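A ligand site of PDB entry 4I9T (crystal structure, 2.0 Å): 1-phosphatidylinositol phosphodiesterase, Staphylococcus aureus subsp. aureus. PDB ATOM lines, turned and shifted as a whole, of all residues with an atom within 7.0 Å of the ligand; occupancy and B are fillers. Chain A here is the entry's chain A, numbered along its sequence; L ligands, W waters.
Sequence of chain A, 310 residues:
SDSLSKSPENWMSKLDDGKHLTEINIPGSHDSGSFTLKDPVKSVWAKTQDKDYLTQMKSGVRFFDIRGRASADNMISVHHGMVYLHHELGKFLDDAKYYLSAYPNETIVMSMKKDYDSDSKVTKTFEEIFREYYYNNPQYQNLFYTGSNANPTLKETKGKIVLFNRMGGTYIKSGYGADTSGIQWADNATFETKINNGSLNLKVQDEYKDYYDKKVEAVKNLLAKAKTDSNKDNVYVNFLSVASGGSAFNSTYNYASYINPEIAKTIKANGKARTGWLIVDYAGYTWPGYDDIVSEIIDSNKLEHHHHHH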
ATOM      1  N   HIS A  30      -9.536 -17.792  31.021  1.00  0.00           N
ATOM      2  CA  HIS A  30     -10.974 -17.877  30.889  1.00  0.00           C
ATOM      3  C   HIS A  30     -11.637 -18.059  32.224  1.00  0.00           C
ATOM      4  O   HIS A  30     -11.176 -18.871  33.044  1.00  0.00           O
ATOM      5  CB  HIS A  30     -11.324 -19.040  29.948  1.00  0.00           C
ATOM      6  CG  HIS A  30     -12.781 -19.418  29.941  1.00  0.00           C
ATOM      7  ND1 HIS A  30     -13.231 -20.549  30.495  1.00  0.00           N
ATOM      8  CD2 HIS A  30     -13.885 -18.769  29.413  1.00  0.00           C
ATOM      9  CE1 HIS A  30     -14.558 -20.627  30.335  1.00  0.00           C
ATOM     10  NE2 HIS A  30     -14.961 -19.534  29.674  1.00  0.00           N
ATOM     11  N   ASP A  31     -12.706 -17.306  32.485  1.00  0.00           N
ATOM     12  CA  ASP A  31     -13.401 -17.399  33.768  1.00  0.00           C
ATOM     13  C   ASP A  31     -12.406 -17.204  34.914  1.00  0.00           C
ATOM     14  O   ASP A  31     -12.359 -17.978  35.861  1.00  0.00           O
ATOM     15  CB  ASP A  31     -14.158 -18.728  33.897  1.00  0.00           C
ATOM     16  CG  ASP A  31     -15.551 -18.680  33.279  1.00  0.00           C
ATOM     17  OD1 ASP A  31     -16.269 -17.687  33.499  1.00  0.00           O
ATOM     18  OD2 ASP A  31     -15.925 -19.627  32.579  1.00  0.00           O
ATOM     19  N   ASP A  65     -10.693 -12.641  31.996  1.00  0.00           N
ATOM     20  CA  ASP A  65     -12.098 -12.768  31.585  1.00  0.00           C
ATOM     21  C   ASP A  65     -12.862 -12.768  32.941  1.00  0.00           C
ATOM     22  O   ASP A  65     -13.074 -13.828  33.591  1.00  0.00           O
ATOM     23  CB  ASP A  65     -12.232 -14.073  30.806  1.00  0.00           C
ATOM     24  CG  ASP A  65     -13.669 -14.461  30.505  1.00  0.00           C
ATOM     25  OD1 ASP A  65     -14.541 -13.585  30.350  1.00  0.00           O
ATOM     26  OD2 ASP A  65     -13.882 -15.691  30.418  1.00  0.00           O
ATOM     27  N   ARG A  67     -16.218 -12.180  35.061  1.00  0.00           N
ATOM     28  CA  ARG A  67     -17.634 -12.289  34.901  1.00  0.00           C
ATOM     29  C   ARG A  67     -18.298 -11.815  36.166  1.00  0.00           C
ATOM     30  O   ARG A  67     -17.924 -12.274  37.276  1.00  0.00           O
ATOM     31  CB  ARG A  67     -18.000 -13.776  34.673  1.00  0.00           C
ATOM     32  CG  ARG A  67     -17.261 -14.416  33.491  1.00  0.00           C
ATOM     33  CD  ARG A  67     -17.614 -13.799  32.117  1.00  0.00           C
ATOM     34  NE  ARG A  67     -16.954 -14.667  31.185  1.00  0.00           N
ATOM     35  CZ  ARG A  67     -17.421 -15.869  30.769  1.00  0.00           C
ATOM     36  NH1 ARG A  67     -18.671 -16.266  31.069  1.00  0.00           N
ATOM     37  NH2 ARG A  67     -16.638 -16.653  30.029  1.00  0.00           N
ATOM     38  N   HIS A  80     -19.402 -17.374  38.128  1.00  0.00           N
ATOM     39  CA  HIS A  80     -19.427 -18.217  36.874  1.00  0.00           C
ATOM     40  C   HIS A  80     -20.900 -18.598  36.720  1.00  0.00           C
ATOM     41  O   HIS A  80     -21.372 -19.563  37.409  1.00  0.00           O
ATOM     42  CB  HIS A  80     -18.551 -19.484  37.053  1.00  0.00           C
ATOM     43  CG  HIS A  80     -18.430 -20.401  35.791  1.00  0.00           C
ATOM     44  ND1 HIS A  80     -19.490 -20.833  35.082  1.00  0.00           N
ATOM     45  CD2 HIS A  80     -17.301 -21.009  35.207  1.00  0.00           C
ATOM     46  CE1 HIS A  80     -19.086 -21.623  34.075  1.00  0.00           C
ATOM     47  NE2 HIS A  80     -17.737 -21.729  34.146  1.00  0.00           N
ATOM     48  N   LYS A 113     -18.063  -8.804  31.688  1.00  0.00           N
ATOM     49  CA  LYS A 113     -19.336  -9.327  31.151  1.00  0.00           C
ATOM     50  C   LYS A 113     -20.278  -9.646  32.327  1.00  0.00           C
ATOM     51  O   LYS A 113     -19.840 -10.177  33.400  1.00  0.00           O
ATOM     52  CB  LYS A 113     -19.030 -10.658  30.497  1.00  0.00           C
ATOM     53  CG  LYS A 113     -20.157 -11.287  29.652  1.00  0.00           C
ATOM     54  CD  LYS A 113     -19.761 -12.734  29.287  1.00  0.00           C
ATOM     55  CE  LYS A 113     -20.889 -13.380  28.489  1.00  0.00           C
ATOM     56  NZ  LYS A 113     -21.771 -14.045  29.463  1.00  0.00           N
ATOM     57  N   ASP A 115     -22.717 -12.057  33.891  1.00  0.00           N
ATOM     58  CA  ASP A 115     -22.858 -13.514  33.787  1.00  0.00           C
ATOM     59  C   ASP A 115     -24.129 -14.125  34.424  1.00  0.00           C
ATOM     60  O   ASP A 115     -24.386 -15.351  34.324  1.00  0.00           O
ATOM     61  CB  ASP A 115     -21.651 -14.198  34.427  1.00  0.00           C
ATOM     62  CG  ASP A 115     -20.995 -15.176  33.461  1.00  0.00           C
ATOM     63  OD1 ASP A 115     -20.944 -14.874  32.251  1.00  0.00           O
ATOM     64  OD2 ASP A 115     -20.585 -16.238  33.898  1.00  0.00           O
ATOM     65  N   ARG A 166     -17.608  -6.432  27.388  1.00  0.00           N
ATOM     66  CA  ARG A 166     -18.588  -7.457  26.960  1.00  0.00           C
ATOM     67  C   ARG A 166     -19.868  -7.229  27.739  1.00  0.00           C
ATOM     68  O   ARG A 166     -20.638  -8.190  28.003  1.00  0.00           O
ATOM     69  CB  ARG A 166     -18.040  -8.870  27.247  1.00  0.00           C
ATOM     70  CG  ARG A 166     -16.942  -9.279  26.225  1.00  0.00           C
ATOM     71  CD  ARG A 166     -16.614 -10.744  26.398  1.00  0.00           C
ATOM     72  NE  ARG A 166     -17.760 -11.573  26.000  1.00  0.00           N
ATOM     73  CZ  ARG A 166     -17.798 -12.896  26.083  1.00  0.00           C
ATOM     74  NH1 ARG A 166     -16.756 -13.629  26.534  1.00  0.00           N
ATOM     75  NH2 ARG A 166     -18.890 -13.522  25.643  1.00  0.00           N
ATOM     76  N   TRP A 185     -21.547 -10.208  20.056  1.00  0.00           N
ATOM     77  CA  TRP A 185     -20.827 -11.467  20.335  1.00  0.00           C
ATOM     78  C   TRP A 185     -21.624 -12.709  19.934  1.00  0.00           C
ATOM     79  O   TRP A 185     -22.596 -13.023  20.582  1.00  0.00           O
ATOM     80  CB  TRP A 185     -20.561 -11.500  21.822  1.00  0.00           C
ATOM     81  CG  TRP A 185     -19.455 -12.457  22.191  1.00  0.00           C
ATOM     82  CD1 TRP A 185     -19.547 -13.838  22.299  1.00  0.00           C
ATOM     83  CD2 TRP A 185     -18.060 -12.110  22.443  1.00  0.00           C
ATOM     84  NE1 TRP A 185     -18.334 -14.390  22.631  1.00  0.00           N
ATOM     85  CE2 TRP A 185     -17.382 -13.382  22.712  1.00  0.00           C
ATOM     86  CE3 TRP A 185     -17.339 -10.926  22.463  1.00  0.00           C
ATOM     87  CZ2 TRP A 185     -16.026 -13.444  23.033  1.00  0.00           C
ATOM     88  CZ3 TRP A 185     -15.965 -10.983  22.761  1.00  0.00           C
ATOM     89  CH2 TRP A 185     -15.324 -12.203  23.017  1.00  0.00           C
ATOM     90  N   ALA A 186     -21.234 -13.456  18.918  1.00  0.00           N
ATOM     91  CA  ALA A 186     -22.056 -14.648  18.479  1.00  0.00           C
ATOM     92  C   ALA A 186     -21.830 -15.833  19.455  1.00  0.00           C
ATOM     93  O   ALA A 186     -20.715 -16.057  19.940  1.00  0.00           O
ATOM     94  CB  ALA A 186     -21.685 -15.037  17.059  1.00  0.00           C
ATOM     95  N   ASP A 187     -22.901 -16.566  19.731  1.00  0.00           N
ATOM     96  CA  ASP A 187     -22.918 -17.612  20.743  1.00  0.00           C
ATOM     97  C   ASP A 187     -22.274 -18.877  20.177  1.00  0.00           C
ATOM     98  O   ASP A 187     -22.649 -19.321  19.089  1.00  0.00           O
ATOM     99  CB  ASP A 187     -24.369 -17.940  21.125  1.00  0.00           C
ATOM    100  CG  ASP A 187     -24.449 -19.005  22.195  1.00  0.00           C
ATOM    101  OD1 ASP A 187     -23.734 -18.960  23.221  1.00  0.00           O
ATOM    102  OD2 ASP A 187     -25.206 -19.931  22.019  1.00  0.00           O
ATOM    103  N   ASN A 188     -21.300 -19.428  20.882  1.00  0.00           N
ATOM    104  CA  ASN A 188     -20.687 -20.699  20.490  1.00  0.00           C
ATOM    105  C   ASN A 188     -20.213 -20.722  19.002  1.00  0.00           C
ATOM    106  O   ASN A 188     -20.629 -21.587  18.216  1.00  0.00           O
ATOM    107  CB  ASN A 188     -21.703 -21.826  20.791  1.00  0.00           C
ATOM    108  CG  ASN A 188     -21.085 -23.194  20.656  1.00  0.00           C
ATOM    109  OD1 ASN A 188     -19.923 -23.385  21.013  1.00  0.00           O
ATOM    110  ND2 ASN A 188     -21.848 -24.171  20.170  1.00  0.00           N
ATOM    111  N   ASP A 206     -14.911 -18.663  19.738  1.00  0.00           N
ATOM    112  CA  ASP A 206     -15.511 -18.889  21.073  1.00  0.00           C
ATOM    113  C   ASP A 206     -16.556 -20.043  21.012  1.00  0.00           C
ATOM    114  O   ASP A 206     -17.705 -19.930  21.468  1.00  0.00           O
ATOM    115  CB  ASP A 206     -16.120 -17.580  21.620  1.00  0.00           C
ATOM    116  CG  ASP A 206     -16.592 -17.722  23.056  1.00  0.00           C
ATOM    117  OD1 ASP A 206     -15.923 -18.435  23.856  1.00  0.00           O
ATOM    118  OD2 ASP A 206     -17.612 -17.098  23.401  1.00  0.00           O
ATOM    119  N   GLU A 207     -16.168 -21.152  20.390  1.00  0.00           N
ATOM    120  CA  GLU A 207     -17.077 -22.306  20.260  1.00  0.00           C
ATOM    121  C   GLU A 207     -16.916 -23.088  21.525  1.00  0.00           C
ATOM    122  O   GLU A 207     -16.303 -24.138  21.532  1.00  0.00           O
ATOM    123  CB  GLU A 207     -16.651 -23.121  19.031  1.00  0.00           C
ATOM    124  CG  GLU A 207     -16.581 -22.282  17.721  1.00  0.00           C
ATOM    125  CD  GLU A 207     -16.148 -23.136  16.505  1.00  0.00           C
ATOM    126  OE1 GLU A 207     -16.209 -24.386  16.597  1.00  0.00           O
ATOM    127  OE2 GLU A 207     -15.718 -22.576  15.453  1.00  0.00           O
ATOM    128  N   TYR A 208     -17.524 -22.588  22.611  1.00  0.00           N
ATOM    129  CA  TYR A 208     -17.322 -23.125  23.950  1.00  0.00           C
ATOM    130  C   TYR A 208     -18.033 -24.459  24.170  1.00  0.00           C
ATOM    131  O   TYR A 208     -17.749 -25.174  25.129  1.00  0.00           O
ATOM    132  CB  TYR A 208     -17.761 -22.111  25.044  1.00  0.00           C
ATOM    133  CG  TYR A 208     -19.257 -21.741  24.999  1.00  0.00           C
ATOM    134  CD1 TYR A 208     -20.183 -22.441  25.792  1.00  0.00           C
ATOM    135  CD2 TYR A 208     -19.716 -20.695  24.221  1.00  0.00           C
ATOM    136  CE1 TYR A 208     -21.533 -22.108  25.793  1.00  0.00           C
ATOM    137  CE2 TYR A 208     -21.055 -20.379  24.166  1.00  0.00           C
ATOM    138  CZ  TYR A 208     -21.954 -21.084  24.940  1.00  0.00           C
ATOM    139  OH  TYR A 208     -23.277 -20.717  24.896  1.00  0.00           O
ATOM    140  N   LYS A 209     -18.943 -24.822  23.276  1.00  0.00           N
ATOM    141  CA  LYS A 209     -19.551 -26.172  23.435  1.00  0.00           C
ATOM    142  C   LYS A 209     -18.884 -27.316  22.631  1.00  0.00           C
ATOM    143  O   LYS A 209     -19.356 -28.464  22.701  1.00  0.00           O
ATOM    144  CB  LYS A 209     -21.019 -26.121  23.117  1.00  0.00           C
ATOM    145  CG  LYS A 209     -21.766 -25.240  24.117  1.00  0.00           C
ATOM    146  CD  LYS A 209     -23.248 -25.491  23.975  1.00  0.00           C
ATOM    147  CE  LYS A 209     -23.875 -24.306  23.275  1.00  0.00           C
ATOM    148  NZ  LYS A 209     -25.318 -24.614  23.349  1.00  0.00           N
ATOM    149  N   LYS A 215     -12.783 -28.607  18.703  1.00  0.00           N
ATOM    150  CA  LYS A 215     -12.273 -27.400  19.387  1.00  0.00           C
ATOM    151  C   LYS A 215     -10.827 -27.153  18.929  1.00  0.00           C
ATOM    152  O   LYS A 215     -10.441 -26.054  18.668  1.00  0.00           O
ATOM    153  CB  LYS A 215     -12.256 -27.583  20.909  1.00  0.00           C
ATOM    154  CG  LYS A 215     -11.790 -26.319  21.586  1.00  0.00           C
ATOM    155  CD  LYS A 215     -12.748 -25.143  21.203  1.00  0.00           C
ATOM    156  CE  LYS A 215     -12.451 -24.022  22.200  1.00  0.00           C
ATOM    157  NZ  LYS A 215     -13.470 -22.929  22.206  1.00  0.00           N
ATOM    158  N   PHE A 239     -10.389 -18.627  22.127  1.00  0.00           N
ATOM    159  CA  PHE A 239     -10.635 -19.250  23.398  1.00  0.00           C
ATOM    160  C   PHE A 239     -10.292 -20.724  23.245  1.00  0.00           C
ATOM    161  O   PHE A 239     -10.813 -21.387  22.320  1.00  0.00           O
ATOM    162  CB  PHE A 239     -12.133 -19.077  23.753  1.00  0.00           C
ATOM    163  CG  PHE A 239     -12.470 -17.723  24.345  1.00  0.00           C
ATOM    164  CD1 PHE A 239     -12.576 -17.544  25.711  1.00  0.00           C
ATOM    165  CD2 PHE A 239     -12.749 -16.635  23.499  1.00  0.00           C
ATOM    166  CE1 PHE A 239     -12.897 -16.261  26.229  1.00  0.00           C
ATOM    167  CE2 PHE A 239     -13.076 -15.373  24.007  1.00  0.00           C
ATOM    168  CZ  PHE A 239     -13.155 -15.185  25.362  1.00  0.00           C
ATOM    169  N   SER A 241     -10.609 -22.754  25.851  1.00  0.00           N
ATOM    170  CA  SER A 241     -11.499 -23.340  26.857  1.00  0.00           C
ATOM    171  C   SER A 241     -12.762 -23.942  26.243  1.00  0.00           C
ATOM    172  O   SER A 241     -13.228 -23.440  25.206  1.00  0.00           O
ATOM    173  CB  SER A 241     -11.975 -22.239  27.844  1.00  0.00           C
ATOM    174  OG  SER A 241     -12.169 -20.978  27.198  1.00  0.00           O
ATOM    175  N   VAL A 242     -13.344 -24.946  26.931  1.00  0.00           N
ATOM    176  CA  VAL A 242     -14.668 -25.485  26.566  1.00  0.00           C
ATOM    177  C   VAL A 242     -15.452 -25.881  27.788  1.00  0.00           C
ATOM    178  O   VAL A 242     -14.886 -26.175  28.813  1.00  0.00           O
ATOM    179  CB  VAL A 242     -14.625 -26.793  25.697  1.00  0.00           C
ATOM    180  CG1 VAL A 242     -14.408 -26.472  24.251  1.00  0.00           C
ATOM    181  CG2 VAL A 242     -13.553 -27.729  26.173  1.00  0.00           C
ATOM    182  N   ALA A 243     -16.762 -25.900  27.656  1.00  0.00           N
ATOM    183  CA  ALA A 243     -17.647 -26.425  28.715  1.00  0.00           C
ATOM    184  C   ALA A 243     -17.472 -27.940  28.947  1.00  0.00           C
ATOM    185  O   ALA A 243     -17.112 -28.671  28.002  1.00  0.00           O
ATOM    186  CB  ALA A 243     -19.086 -26.044  28.415  1.00  0.00           C
HETATM  187  C1  LIG L   1     -19.618 -19.647  27.998  1.00  0.00           C
HETATM  188  C2  LIG L   1     -18.106 -19.633  27.670  1.00  0.00           C
HETATM  189  C3  LIG L   1     -17.709 -18.592  26.646  1.00  0.00           C
HETATM  190  C4  LIG L   1     -18.292 -17.226  26.968  1.00  0.00           C
HETATM  191  C5  LIG L   1     -19.806 -17.411  26.877  1.00  0.00           C
HETATM  192  C6  LIG L   1     -20.215 -18.246  28.102  1.00  0.00           C
HETATM  193  O1  LIG L   1     -19.688 -20.230  29.293  1.00  0.00           O
HETATM  194  O2  LIG L   1     -17.489 -19.302  28.930  1.00  0.00           O
HETATM  195  O3  LIG L   1     -16.281 -18.494  26.570  1.00  0.00           O
HETATM  196  O4  LIG L   1     -17.897 -16.366  25.907  1.00  0.00           O
HETATM  197  O5  LIG L   1     -20.462 -16.116  26.765  1.00  0.00           O
HETATM  198  O6  LIG L   1     -21.648 -18.339  28.136  1.00  0.00           O
HETATM  199  O   HOH W   1     -18.483 -19.047  31.326  1.00  0.00           O
HETATM  200  O   HOH W   2     -21.745 -16.327  24.133  1.00  0.00           O
HETATM  201  O   HOH W   3     -14.808 -20.979  26.604  1.00  0.00           O
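The side-chain carboxylate of Asp 206 is in hydrogen-bond range of the indole nitrogen of Trp 185, at 2.9 Å.
A ring nitrogen (NE2) of His 80 lies within hydrogen-bond range of the side-chain carboxylate (OD2) of Asp 31.
OD1 of Asp 115 lies within salt-bridge range of NH1 of Arg 67, at 2.9 Å.
O of Phe 239 is in hydrogen-bond range of NZ of Lys 215, at 3.1 Å.
The guanidinium group of Arg 67 is in salt-bridge range of the side-chain carboxylate of Asp 65 (2.8 Å).
NE2 of His 30 lies within hydrogen-bond range of NH2 of Arg 67 (3.4 Å).
The side-chain carboxylate of Asp 115 is in salt-bridge range of the side-chain amino group of Lys 113.
OD1 of Asp 187 sits at hydrogen-bond distance from OH of Tyr 208 (2.5 Å).
Merely in contact with the ligand: Lys 113, Tyr 208, Trp 185, Phe 239 and Asp 31.
The nearest printed residue that does not touch the ligand is Ser 241 (4.8 Å).
An oxygen (O4) of the ligand is in hydrogen-bond range of the side-chain carboxylate of Asp 206 (2.6 Å).
An oxygen (O4) of the ligand lies within hydrogen-bond range of the guanidinium group (NH2) of Arg 166.
O2 of the ligand lies within hydrogen-bond range of NH2 of Arg 67, at 3.0 Å.
NE2 of His 30 is in hydrogen-bond range of O2 of the ligand (2.6 Å).
Water W1 lies within hydrogen-bond range of O2 of the ligand, NH1 of Arg 67 and OD2 of Asp 31.
Water W3 lies within hydrogen-bond range of OG of Ser 241 (2.7 Å), O3 of the ligand (2.9 Å) and NE2 of His 30 (3.4 Å).
Water W2 lies within hydrogen-bond range of an oxygen (O5) of the ligand (2.9 Å) and the side-chain carboxylate (OD1) of Asp 187 (3.4 Å).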
